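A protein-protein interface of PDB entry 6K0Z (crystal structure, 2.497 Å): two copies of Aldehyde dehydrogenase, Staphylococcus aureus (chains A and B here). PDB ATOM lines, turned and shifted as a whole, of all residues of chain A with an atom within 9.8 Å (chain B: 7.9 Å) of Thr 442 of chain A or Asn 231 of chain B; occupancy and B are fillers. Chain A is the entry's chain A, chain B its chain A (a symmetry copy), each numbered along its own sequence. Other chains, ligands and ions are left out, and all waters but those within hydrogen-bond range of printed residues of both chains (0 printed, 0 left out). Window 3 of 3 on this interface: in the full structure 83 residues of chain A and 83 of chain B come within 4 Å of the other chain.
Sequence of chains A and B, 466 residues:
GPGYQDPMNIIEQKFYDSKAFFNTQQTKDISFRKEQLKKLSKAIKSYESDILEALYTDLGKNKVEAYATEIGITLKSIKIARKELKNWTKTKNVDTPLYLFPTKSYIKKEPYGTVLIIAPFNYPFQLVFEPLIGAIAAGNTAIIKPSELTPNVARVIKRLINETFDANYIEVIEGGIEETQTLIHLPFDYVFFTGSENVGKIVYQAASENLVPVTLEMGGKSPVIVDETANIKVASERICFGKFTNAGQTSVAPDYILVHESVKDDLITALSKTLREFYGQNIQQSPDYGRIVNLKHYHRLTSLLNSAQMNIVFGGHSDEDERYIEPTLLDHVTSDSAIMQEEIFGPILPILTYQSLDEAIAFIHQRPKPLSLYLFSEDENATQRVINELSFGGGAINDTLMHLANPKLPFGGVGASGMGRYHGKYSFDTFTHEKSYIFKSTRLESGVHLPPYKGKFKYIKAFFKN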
ATOM      1  N   PRO A 102      32.197   6.790 -17.894  1.00  0.00           N
ATOM      2  CA  PRO A 102      33.338   5.854 -17.931  1.00  0.00           C
ATOM      3  C   PRO A 102      34.118   5.733 -19.256  1.00  0.00           C
ATOM      4  O   PRO A 102      34.912   4.792 -19.409  1.00  0.00           O
ATOM      5  CB  PRO A 102      32.665   4.512 -17.624  1.00  0.00           C
ATOM      6  CG  PRO A 102      31.318   4.638 -18.285  1.00  0.00           C
ATOM      7  CD  PRO A 102      30.944   6.111 -18.271  1.00  0.00           C
ATOM      8  N   THR A 103      33.899   6.667 -20.185  1.00  0.00           N
ATOM      9  CA  THR A 103      34.493   6.597 -21.516  1.00  0.00           C
ATOM     10  C   THR A 103      35.996   6.348 -21.434  1.00  0.00           C
ATOM     11  O   THR A 103      36.692   6.937 -20.602  1.00  0.00           O
ATOM     12  CB  THR A 103      34.210   7.905 -22.278  1.00  0.00           C
ATOM     13  OG1 THR A 103      32.812   8.240 -22.171  1.00  0.00           O
ATOM     14  CG2 THR A 103      34.571   7.780 -23.745  1.00  0.00           C
ATOM     15  N   LYS A 104      36.488   5.448 -22.287  1.00  0.00           N
ATOM     16  CA  LYS A 104      37.913   5.216 -22.463  1.00  0.00           C
ATOM     17  C   LYS A 104      38.404   5.961 -23.698  1.00  0.00           C
ATOM     18  O   LYS A 104      37.657   6.161 -24.653  1.00  0.00           O
ATOM     19  CB  LYS A 104      38.221   3.718 -22.606  1.00  0.00           C
ATOM     20  N   PHE A 439      35.787   4.766 -26.211  1.00  0.00           N
ATOM     21  CA  PHE A 439      35.021   3.555 -25.945  1.00  0.00           C
ATOM     22  C   PHE A 439      34.172   3.824 -24.709  1.00  0.00           C
ATOM     23  O   PHE A 439      34.703   3.883 -23.594  1.00  0.00           O
ATOM     24  CB  PHE A 439      35.947   2.354 -25.748  1.00  0.00           C
ATOM     25  CG  PHE A 439      35.301   1.188 -25.037  1.00  0.00           C
ATOM     26  CD1 PHE A 439      34.100   0.653 -25.487  1.00  0.00           C
ATOM     27  CD2 PHE A 439      35.904   0.621 -23.920  1.00  0.00           C
ATOM     28  CE1 PHE A 439      33.507  -0.416 -24.832  1.00  0.00           C
ATOM     29  CE2 PHE A 439      35.315  -0.453 -23.264  1.00  0.00           C
ATOM     30  CZ  PHE A 439      34.116  -0.971 -23.723  1.00  0.00           C
ATOM     31  N   LYS A 440      32.867   4.010 -24.911  1.00  0.00           N
ATOM     32  CA  LYS A 440      31.929   4.294 -23.830  1.00  0.00           C
ATOM     33  C   LYS A 440      31.026   3.085 -23.649  1.00  0.00           C
ATOM     34  O   LYS A 440      30.124   2.846 -24.461  1.00  0.00           O
ATOM     35  CB  LYS A 440      31.104   5.545 -24.109  1.00  0.00           C
ATOM     36  CG  LYS A 440      30.185   5.905 -22.958  1.00  0.00           C
ATOM     37  CD  LYS A 440      29.293   7.071 -23.302  1.00  0.00           C
ATOM     38  CE  LYS A 440      28.622   7.625 -22.066  1.00  0.00           C
ATOM     39  NZ  LYS A 440      27.384   8.364 -22.421  1.00  0.00           N
ATOM     40  N   SER A 441      31.267   2.334 -22.581  1.00  0.00           N
ATOM     41  CA  SER A 441      30.478   1.144 -22.310  1.00  0.00           C
ATOM     42  C   SER A 441      28.999   1.486 -22.158  1.00  0.00           C
ATOM     43  O   SER A 441      28.627   2.595 -21.768  1.00  0.00           O
ATOM     44  CB  SER A 441      30.981   0.465 -21.042  1.00  0.00           C
ATOM     45  OG  SER A 441      29.973  -0.362 -20.495  1.00  0.00           O
ATOM     46  N   THR A 442      28.150   0.503 -22.461  1.00  0.00           N
ATOM     47  CA  THR A 442      26.705   0.678 -22.436  1.00  0.00           C
ATOM     48  C   THR A 442      26.052   0.167 -21.154  1.00  0.00           C
ATOM     49  O   THR A 442      24.845   0.374 -20.979  1.00  0.00           O
ATOM     50  CB  THR A 442      26.070  -0.028 -23.638  1.00  0.00           C
ATOM     51  OG1 THR A 442      26.435  -1.411 -23.622  1.00  0.00           O
ATOM     52  CG2 THR A 442      26.556   0.584 -24.928  1.00  0.00           C
ATOM     53  N   ARG A 443      26.808  -0.496 -20.266  1.00  0.00           N
ATOM     54  CA  ARG A 443      26.232  -0.995 -19.020  1.00  0.00           C
ATOM     55  C   ARG A 443      25.761   0.160 -18.139  1.00  0.00           C
ATOM     56  O   ARG A 443      24.625   0.176 -17.658  1.00  0.00           O
ATOM     57  CB  ARG A 443      27.249  -1.879 -18.278  1.00  0.00           C
ATOM     58  CG  ARG A 443      27.755  -3.061 -19.133  1.00  0.00           C
ATOM     59  CD  ARG A 443      29.146  -3.586 -18.715  1.00  0.00           C
ATOM     60  NE  ARG A 443      30.021  -3.846 -19.859  1.00  0.00           N
ATOM     61  CZ  ARG A 443      31.112  -3.118 -20.137  1.00  0.00           C
ATOM     62  NH1 ARG A 443      31.483  -2.097 -19.353  1.00  0.00           N
ATOM     63  NH2 ARG A 443      31.865  -3.398 -21.204  1.00  0.00           N
ATOM     64  N   LEU A 444      26.636   1.133 -17.907  1.00  0.00           N
ATOM     65  CA  LEU A 444      26.291   2.362 -17.186  1.00  0.00           C
ATOM     66  C   LEU A 444      25.908   3.431 -18.212  1.00  0.00           C
ATOM     67  O   LEU A 444      26.749   4.201 -18.683  1.00  0.00           O
ATOM     68  CB  LEU A 444      27.447   2.826 -16.292  1.00  0.00           C
ATOM     69  CG  LEU A 444      27.820   1.934 -15.104  1.00  0.00           C
ATOM     70  CD1 LEU A 444      28.969   2.559 -14.324  1.00  0.00           C
ATOM     71  CD2 LEU A 444      26.631   1.654 -14.181  1.00  0.00           C
ATOM     72  N   GLU A 445      24.628   3.461 -18.570  1.00  0.00           N
ATOM     73  CA  GLU A 445      24.078   4.523 -19.399  1.00  0.00           C
ATOM     74  C   GLU A 445      23.565   5.672 -18.527  1.00  0.00           C
ATOM     75  O   GLU A 445      23.344   5.521 -17.322  1.00  0.00           O
ATOM     76  CB  GLU A 445      22.949   3.988 -20.282  1.00  0.00           C
ATOM     77  N   SER A 446      23.389   6.845 -19.125  1.00  0.00           N
ATOM     78  CA  SER A 446      22.990   8.004 -18.341  1.00  0.00           C
ATOM     79  C   SER A 446      21.978   8.892 -19.020  1.00  0.00           C
ATOM     80  O   SER A 446      20.901   8.449 -19.362  1.00  0.00           O
ATOM     81  CB  SER A 446      24.225   8.815 -17.972  1.00  0.00           C
ATOM     82  OG  SER A 446      24.395   8.897 -16.572  1.00  0.00           O
ATOM     83  N   VAL B 226      26.111  -0.823 -36.736  1.00  0.00           N
ATOM     84  CA  VAL B 226      25.299  -1.358 -35.649  1.00  0.00           C
ATOM     85  C   VAL B 226      25.269  -2.871 -35.812  1.00  0.00           C
ATOM     86  O   VAL B 226      24.661  -3.402 -36.748  1.00  0.00           O
ATOM     87  CB  VAL B 226      23.889  -0.756 -35.642  1.00  0.00           C
ATOM     88  CG1 VAL B 226      23.132  -1.220 -34.413  1.00  0.00           C
ATOM     89  CG2 VAL B 226      23.979   0.770 -35.677  1.00  0.00           C
ATOM     90  N   ASP B 227      25.921  -3.562 -34.888  1.00  0.00           N
ATOM     91  CA  ASP B 227      26.326  -4.947 -35.054  1.00  0.00           C
ATOM     92  C   ASP B 227      25.336  -5.890 -34.376  1.00  0.00           C
ATOM     93  O   ASP B 227      24.586  -5.501 -33.478  1.00  0.00           O
ATOM     94  CB  ASP B 227      27.739  -5.117 -34.490  1.00  0.00           C
ATOM     95  CG  ASP B 227      28.292  -6.505 -34.669  1.00  0.00           C
ATOM     96  OD1 ASP B 227      28.431  -6.958 -35.830  1.00  0.00           O
ATOM     97  OD2 ASP B 227      28.626  -7.126 -33.636  1.00  0.00           O
ATOM     98  N   GLU B 228      25.345  -7.149 -34.834  1.00  0.00           N
ATOM     99  CA  GLU B 228      24.417  -8.168 -34.344  1.00  0.00           C
ATOM    100  C   GLU B 228      24.402  -8.282 -32.824  1.00  0.00           C
ATOM    101  O   GLU B 228      23.408  -8.746 -32.258  1.00  0.00           O
ATOM    102  CB  GLU B 228      24.770  -9.525 -34.972  1.00  0.00           C
ATOM    103  CG  GLU B 228      26.203  -9.981 -34.697  1.00  0.00           C
ATOM    104  CD  GLU B 228      26.570 -11.285 -35.394  1.00  0.00           C
ATOM    105  OE1 GLU B 228      25.666 -11.969 -35.922  1.00  0.00           O
ATOM    106  OE2 GLU B 228      27.771 -11.630 -35.411  1.00  0.00           O
ATOM    107  N   THR B 229      25.469  -7.863 -32.146  1.00  0.00           N
ATOM    108  CA  THR B 229      25.564  -7.973 -30.698  1.00  0.00           C
ATOM    109  C   THR B 229      25.290  -6.652 -29.988  1.00  0.00           C
ATOM    110  O   THR B 229      25.686  -6.490 -28.829  1.00  0.00           O
ATOM    111  CB  THR B 229      26.948  -8.492 -30.309  1.00  0.00           C
ATOM    112  OG1 THR B 229      27.862  -7.389 -30.241  1.00  0.00           O
ATOM    113  CG2 THR B 229      27.454  -9.477 -31.346  1.00  0.00           C
ATOM    114  N   ALA B 230      24.618  -5.710 -30.645  1.00  0.00           N
ATOM    115  CA  ALA B 230      24.576  -4.344 -30.141  1.00  0.00           C
ATOM    116  C   ALA B 230      23.593  -4.188 -28.984  1.00  0.00           C
ATOM    117  O   ALA B 230      22.736  -5.035 -28.737  1.00  0.00           O
ATOM    118  CB  ALA B 230      24.196  -3.368 -31.255  1.00  0.00           C
ATOM    119  N   ASN B 231      23.700  -3.065 -28.313  1.00  0.00           N
ATOM    120  CA  ASN B 231      22.763  -2.747 -27.290  1.00  0.00           C
ATOM    121  C   ASN B 231      21.914  -1.733 -27.971  1.00  0.00           C
ATOM    122  O   ASN B 231      22.050  -0.575 -27.744  1.00  0.00           O
ATOM    123  CB  ASN B 231      23.428  -2.139 -26.074  1.00  0.00           C
ATOM    124  CG  ASN B 231      22.427  -1.661 -25.043  1.00  0.00           C
ATOM    125  OD1 ASN B 231      21.354  -1.173 -25.367  1.00  0.00           O
ATOM    126  ND2 ASN B 231      22.789  -1.798 -23.793  1.00  0.00           N
ATOM    127  N   ILE B 232      20.976  -2.163 -28.785  1.00  0.00           N
ATOM    128  CA  ILE B 232      20.120  -1.240 -29.534  1.00  0.00           C
ATOM    129  C   ILE B 232      19.477  -0.054 -28.815  1.00  0.00           C
ATOM    130  O   ILE B 232      19.276   0.969 -29.411  1.00  0.00           O
ATOM    131  CB  ILE B 232      19.029  -2.002 -30.317  1.00  0.00           C
ATOM    132  CG1 ILE B 232      19.652  -2.948 -31.316  1.00  0.00           C
ATOM    133  CG2 ILE B 232      18.145  -1.044 -31.074  1.00  0.00           C
ATOM    134  CD1 ILE B 232      20.340  -4.113 -30.672  1.00  0.00           C
ATOM    135  N   LYS B 233      19.115  -0.214 -27.553  1.00  0.00           N
ATOM    136  CA  LYS B 233      18.490   0.822 -26.766  1.00  0.00           C
ATOM    137  C   LYS B 233      19.351   2.045 -26.561  1.00  0.00           C
ATOM    138  O   LYS B 233      18.942   3.146 -26.875  1.00  0.00           O
ATOM    139  CB  LYS B 233      18.088   0.254 -25.409  1.00  0.00           C
ATOM    140  N   VAL B 234      20.536   1.849 -26.012  1.00  0.00           N
ATOM    141  CA  VAL B 234      21.402   2.968 -25.762  1.00  0.00           C
ATOM    142  C   VAL B 234      21.971   3.523 -27.060  1.00  0.00           C
ATOM    143  O   VAL B 234      22.106   4.736 -27.220  1.00  0.00           O
ATOM    144  CB  VAL B 234      22.462   2.655 -24.707  1.00  0.00           C
ATOM    145  CG1 VAL B 234      21.803   2.012 -23.520  1.00  0.00           C
ATOM    146  CG2 VAL B 234      23.558   1.759 -25.238  1.00  0.00           C
ATOM    147  N   ALA B 235      22.221   2.652 -28.032  1.00  0.00           N
ATOM    148  CA  ALA B 235      22.774   3.078 -29.285  1.00  0.00           C
ATOM    149  C   ALA B 235      21.797   3.965 -29.973  1.00  0.00           C
ATOM    150  O   ALA B 235      22.157   4.889 -30.647  1.00  0.00           O
ATOM    151  CB  ALA B 235      23.117   1.894 -30.144  1.00  0.00           C
ATOM    152  N   SER B 236      20.533   3.740 -29.749  1.00  0.00           N
ATOM    153  CA  SER B 236      19.549   4.563 -30.404  1.00  0.00           C
ATOM    154  C   SER B 236      19.642   6.000 -29.953  1.00  0.00           C
ATOM    155  O   SER B 236      19.520   6.913 -30.747  1.00  0.00           O
ATOM    156  CB  SER B 236      18.167   4.014 -30.126  1.00  0.00           C
ATOM    157  OG  SER B 236      17.777   4.316 -28.803  1.00  0.00           O
ATOM    158  N   GLU B 237      19.840   6.183 -28.659  1.00  0.00           N
ATOM    159  CA  GLU B 237      19.965   7.487 -28.059  1.00  0.00           C
ATOM    160  C   GLU B 237      21.294   8.097 -28.458  1.00  0.00           C
ATOM    161  O   GLU B 237      21.343   9.181 -28.985  1.00  0.00           O
ATOM    162  CB  GLU B 237      19.908   7.356 -26.539  1.00  0.00           C
ATOM    163  CG  GLU B 237      18.520   7.156 -25.957  1.00  0.00           C
ATOM    164  CD  GLU B 237      18.538   6.475 -24.603  1.00  0.00           C
ATOM    165  OE1 GLU B 237      19.612   6.114 -24.102  1.00  0.00           O
ATOM    166  OE2 GLU B 237      17.465   6.302 -24.041  1.00  0.00           O
ATOM    167  N   ARG B 238      22.371   7.372 -28.210  1.00  0.00           N
ATOM    168  CA  ARG B 238      23.697   7.838 -28.553  1.00  0.00           C
ATOM    169  C   ARG B 238      23.821   8.270 -30.014  1.00  0.00           C
ATOM    170  O   ARG B 238      24.333   9.313 -30.292  1.00  0.00           O
ATOM    171  CB  ARG B 238      24.746   6.802 -28.174  1.00  0.00           C
ATOM    172  CG  ARG B 238      25.120   6.850 -26.712  1.00  0.00           C
ATOM    173  CD  ARG B 238      26.120   5.799 -26.285  1.00  0.00           C
ATOM    174  NE  ARG B 238      26.047   5.576 -24.849  1.00  0.00           N
ATOM    175  CZ  ARG B 238      26.839   4.765 -24.159  1.00  0.00           C
ATOM    176  NH1 ARG B 238      27.787   4.074 -24.741  1.00  0.00           N
ATOM    177  NH2 ARG B 238      26.682   4.646 -22.867  1.00  0.00           N
ATOM    178  N   VAL B 263      18.948  -7.146 -36.743  1.00  0.00           N
ATOM    179  CA  VAL B 263      18.523  -6.116 -35.795  1.00  0.00           C
ATOM    180  C   VAL B 263      17.919  -4.890 -36.466  1.00  0.00           C
ATOM    181  O   VAL B 263      17.538  -3.938 -35.772  1.00  0.00           O
ATOM    182  CB  VAL B 263      19.706  -5.659 -34.921  1.00  0.00           C
ATOM    183  CG1 VAL B 263      20.302  -6.839 -34.170  1.00  0.00           C
ATOM    184  CG2 VAL B 263      20.750  -5.002 -35.789  1.00  0.00           C
ATOM    185  N   LEU B 267      16.038  -1.446 -34.412  1.00  0.00           N
ATOM    186  CA  LEU B 267      16.657  -0.150 -34.370  1.00  0.00           C
ATOM    187  C   LEU B 267      15.719   0.955 -34.660  1.00  0.00           C
ATOM    188  O   LEU B 267      15.641   1.905 -33.927  1.00  0.00           O
ATOM    189  CB  LEU B 267      17.786  -0.087 -35.376  1.00  0.00           C
ATOM    190  CG  LEU B 267      18.466   1.258 -35.573  1.00  0.00           C
ATOM    191  CD1 LEU B 267      19.186   1.632 -34.305  1.00  0.00           C
ATOM    192  CD2 LEU B 267      19.454   1.173 -36.710  1.00  0.00           C
ATOM    193  N   ALA B 270      13.383   1.619 -31.890  1.00  0.00           N
ATOM    194  CA  ALA B 270      14.213   2.103 -30.815  1.00  0.00           C
ATOM    195  C   ALA B 270      14.619   3.520 -31.096  1.00  0.00           C
ATOM    196  O   ALA B 270      14.645   4.339 -30.212  1.00  0.00           O
ATOM    197  CB  ALA B 270      15.438   1.232 -30.653  1.00  0.00           C
ATOM    198  N   PHE B 376      28.732   0.288 -33.017  1.00  0.00           N
ATOM    199  CA  PHE B 376      27.958  -0.111 -31.848  1.00  0.00           C
ATOM    200  C   PHE B 376      27.943  -1.634 -31.805  1.00  0.00           C
ATOM    201  O   PHE B 376      27.228  -2.282 -32.574  1.00  0.00           O
ATOM    202  CB  PHE B 376      26.561   0.496 -31.896  1.00  0.00           C
ATOM    203  CG  PHE B 376      26.531   1.935 -31.477  1.00  0.00           C
ATOM    204  CD1 PHE B 376      26.489   2.276 -30.134  1.00  0.00           C
ATOM    205  CD2 PHE B 376      26.585   2.946 -32.419  1.00  0.00           C
ATOM    206  CE1 PHE B 376      26.472   3.599 -29.741  1.00  0.00           C
ATOM    207  CE2 PHE B 376      26.578   4.273 -32.026  1.00  0.00           C
ATOM    208  CZ  PHE B 376      26.516   4.599 -30.690  1.00  0.00           C
ATOM    209  N   SER B 377      28.761  -2.196 -30.918  1.00  0.00           N
ATOM    210  CA  SER B 377      28.904  -3.639 -30.803  1.00  0.00           C
ATOM    211  C   SER B 377      29.452  -3.981 -29.429  1.00  0.00           C
ATOM    212  O   SER B 377      30.235  -3.222 -28.846  1.00  0.00           O
ATOM    213  CB  SER B 377      29.833  -4.210 -31.874  1.00  0.00           C
ATOM    214  OG  SER B 377      30.257  -5.518 -31.520  1.00  0.00           O
ATOM    215  N   GLU B 378      29.036  -5.143 -28.932  1.00  0.00           N
ATOM    216  CA  GLU B 378      29.573  -5.708 -27.705  1.00  0.00           C
ATOM    217  C   GLU B 378      30.608  -6.790 -27.963  1.00  0.00           C
ATOM    218  O   GLU B 378      31.155  -7.348 -27.004  1.00  0.00           O
ATOM    219  CB  GLU B 378      28.444  -6.280 -26.838  1.00  0.00           C
ATOM    220  CG  GLU B 378      27.486  -5.241 -26.263  1.00  0.00           C
ATOM    221  CD  GLU B 378      28.189  -4.204 -25.392  1.00  0.00           C
ATOM    222  OE1 GLU B 378      27.627  -3.113 -25.190  1.00  0.00           O
ATOM    223  OE2 GLU B 378      29.299  -4.477 -24.896  1.00  0.00           O
ATOM    224  N   ILE B 397      33.756   3.722 -30.351  1.00  0.00           N
ATOM    225  CA  ILE B 397      33.098   2.442 -30.150  1.00  0.00           C
ATOM    226  C   ILE B 397      32.013   2.646 -29.103  1.00  0.00           C
ATOM    227  O   ILE B 397      32.303   3.040 -27.967  1.00  0.00           O
ATOM    228  CB  ILE B 397      34.093   1.365 -29.706  1.00  0.00           C
ATOM    229  CG1 ILE B 397      35.201   1.231 -30.739  1.00  0.00           C
ATOM    230  CG2 ILE B 397      33.370   0.031 -29.530  1.00  0.00           C
ATOM    231  CD1 ILE B 397      34.691   0.964 -32.149  1.00  0.00           C
ATOM    232  N   ASN B 398      30.766   2.382 -29.491  1.00  0.00           N
ATOM    233  CA  ASN B 398      29.612   2.480 -28.597  1.00  0.00           C
ATOM    234  C   ASN B 398      29.382   3.909 -28.125  1.00  0.00           C
ATOM    235  O   ASN B 398      29.098   4.149 -26.950  1.00  0.00           O
ATOM    236  CB  ASN B 398      29.748   1.537 -27.405  1.00  0.00           C
ATOM    237  CG  ASN B 398      29.511   0.111 -27.787  1.00  0.00           C
ATOM    238  OD1 ASN B 398      28.565  -0.195 -28.511  1.00  0.00           O
ATOM    239  ND2 ASN B 398      30.375  -0.778 -27.317  1.00  0.00           N
ATOM    240  N   ASP B 399      29.489   4.856 -29.053  1.00  0.00           N
ATOM    241  CA  ASP B 399      29.190   6.266 -28.820  1.00  0.00           C
ATOM    242  C   ASP B 399      29.358   6.987 -30.153  1.00  0.00           C
ATOM    243  O   ASP B 399      29.892   6.429 -31.114  1.00  0.00           O
ATOM    244  CB  ASP B 399      30.090   6.898 -27.752  1.00  0.00           C
ATOM    245  CG  ASP B 399      29.432   8.077 -27.059  1.00  0.00           C
ATOM    246  OD1 ASP B 399      28.468   8.636 -27.619  1.00  0.00           O
ATOM    247  OD2 ASP B 399      29.880   8.455 -25.957  1.00  0.00           O
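The guanidinium group (NH1) of Arg 238 of chain B is in hydrogen-bond range of the backbone carbonyl oxygen (O) of Lys 440 of chain A (2.7 Å). O of Ile 397 of chain B sits at hydrogen-bond distance from N of Lys 440 of chain A. The guanidinium group (NH2) of Arg 238 of chain B lies within hydrogen-bond range of the backbone carbonyl oxygen (O) of Ser 441 of chain A (3.0 Å). OE1 of Glu 378 of chain B is in hydrogen-bond range of OG1 of Thr 442 of chain A (2.6 Å). O of Asn 398 of chain B sits close to O of Lys 440 of chain A, 3.0 Å away.
The backbone carbonyl oxygen of Phe 439 of chain A is in hydrogen-bond range of the backbone NH of Lys 104 of chain A (2.7 Å). The guanidinium group (NH1) of Arg 443 of chain A lies within hydrogen-bond range of the side-chain hydroxyl (OG) of Ser 441 of chain A (2.6 Å). The backbone NH (N) of Glu 378 of chain B is in hydrogen-bond range of the side-chain hydroxyl (OG1) of Thr 229 of chain B (2.9 Å). The backbone NH (N) of Val 234 of chain B sits at hydrogen-bond distance from the side-chain amide oxygen (OD1) of Asn 231 of chain B (3.2 Å). The guanidinium group (NH1) of Arg 238 of chain B is in hydrogen-bond range of the backbone carbonyl oxygen (O) of Asn 398 of chain B (2.6 Å). O of Ser 377 of chain B sits at hydrogen-bond distance from ND2 of Asn 398 of chain B, at 2.9 Å.
Phe 439 of chain A touches Ile 397 of chain B (CA to O, 3.4 Å). OD2 of Asp 399 of chain B touches CD of Lys 440 of chain A, 3.1 Å away. Asn 231 of chain B touches Thr 442 of chain A. Thr 442 of chain A touches Val 234 of chain B (CG2 to CG2, 3.2 Å). Arg 238 of chain B touches Thr 442 of chain A. Val 234 of chain B touches Glu 445 of chain A (CG1 to CB, 3.96 Å).
Of chain B, only Arg 238 comes within 4 Å of Ser 441 of chain A. Thr 442 of chain A touches just these residues of chain B: Asn 231 (3.7 Å), Val 234 (3.2 Å), Arg 238 (3.7 Å) and Glu 378 (2.6 Å). Of the printed residues of chain B, Glu 445 of chain A touches Val 234. Thr 229 of chain B touches none of the printed residues of chain A. No residue of chain A comes within 4 Å of Ala 230 of chain B. Asn 231 of chain B touches just one residue of chain A: Thr 442 (3.7 Å). Ile 232 of chain B touches none of the printed residues of chain A. Lys 233 of chain B touches none of the printed residues of chain A. Val 234 of chain B touches two residues of chain A. Ser 377 of chain B touches none of the printed residues of chain A. Of the printed residues of chain A, Ile 397 of chain B touches Phe 439 and Lys 440. The nearest residue of chain A that does not touch Asn 231 of chain B is Arg 443 of chain A (5.5 Å). The nearest printed residue of chain A that does not touch Asn 398 of chain B is Phe 439 of chain A (4.01 Å).
Of the 11 printed residues of chain A, 5 touch a printed residue of chain B. Printed residues of chain A that touch a printed residue of chain B: Phe 439, Lys 440, Ser 441, Thr 442 and Glu 445. Hydrophobic or aromatic side chains of chain A that line the printed part of chain B: Phe 439. Printed residues of chain B that touch a printed residue of chain A: Asn 231, Val 234, Arg 238, Glu 378, Ile 397, Asn 398 and Asp 399. Among the printed residues, 11 pairs touch across the chains. Among the printed residues, no Asp or Glu carboxylate lies within 4 Å of a Lys or Arg side-chain nitrogen of the other chain.
No position is printed for both chains. Of the 11 pairs that touch across the chains among the printed residues, none has its exchanged pair printed and touching as well.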
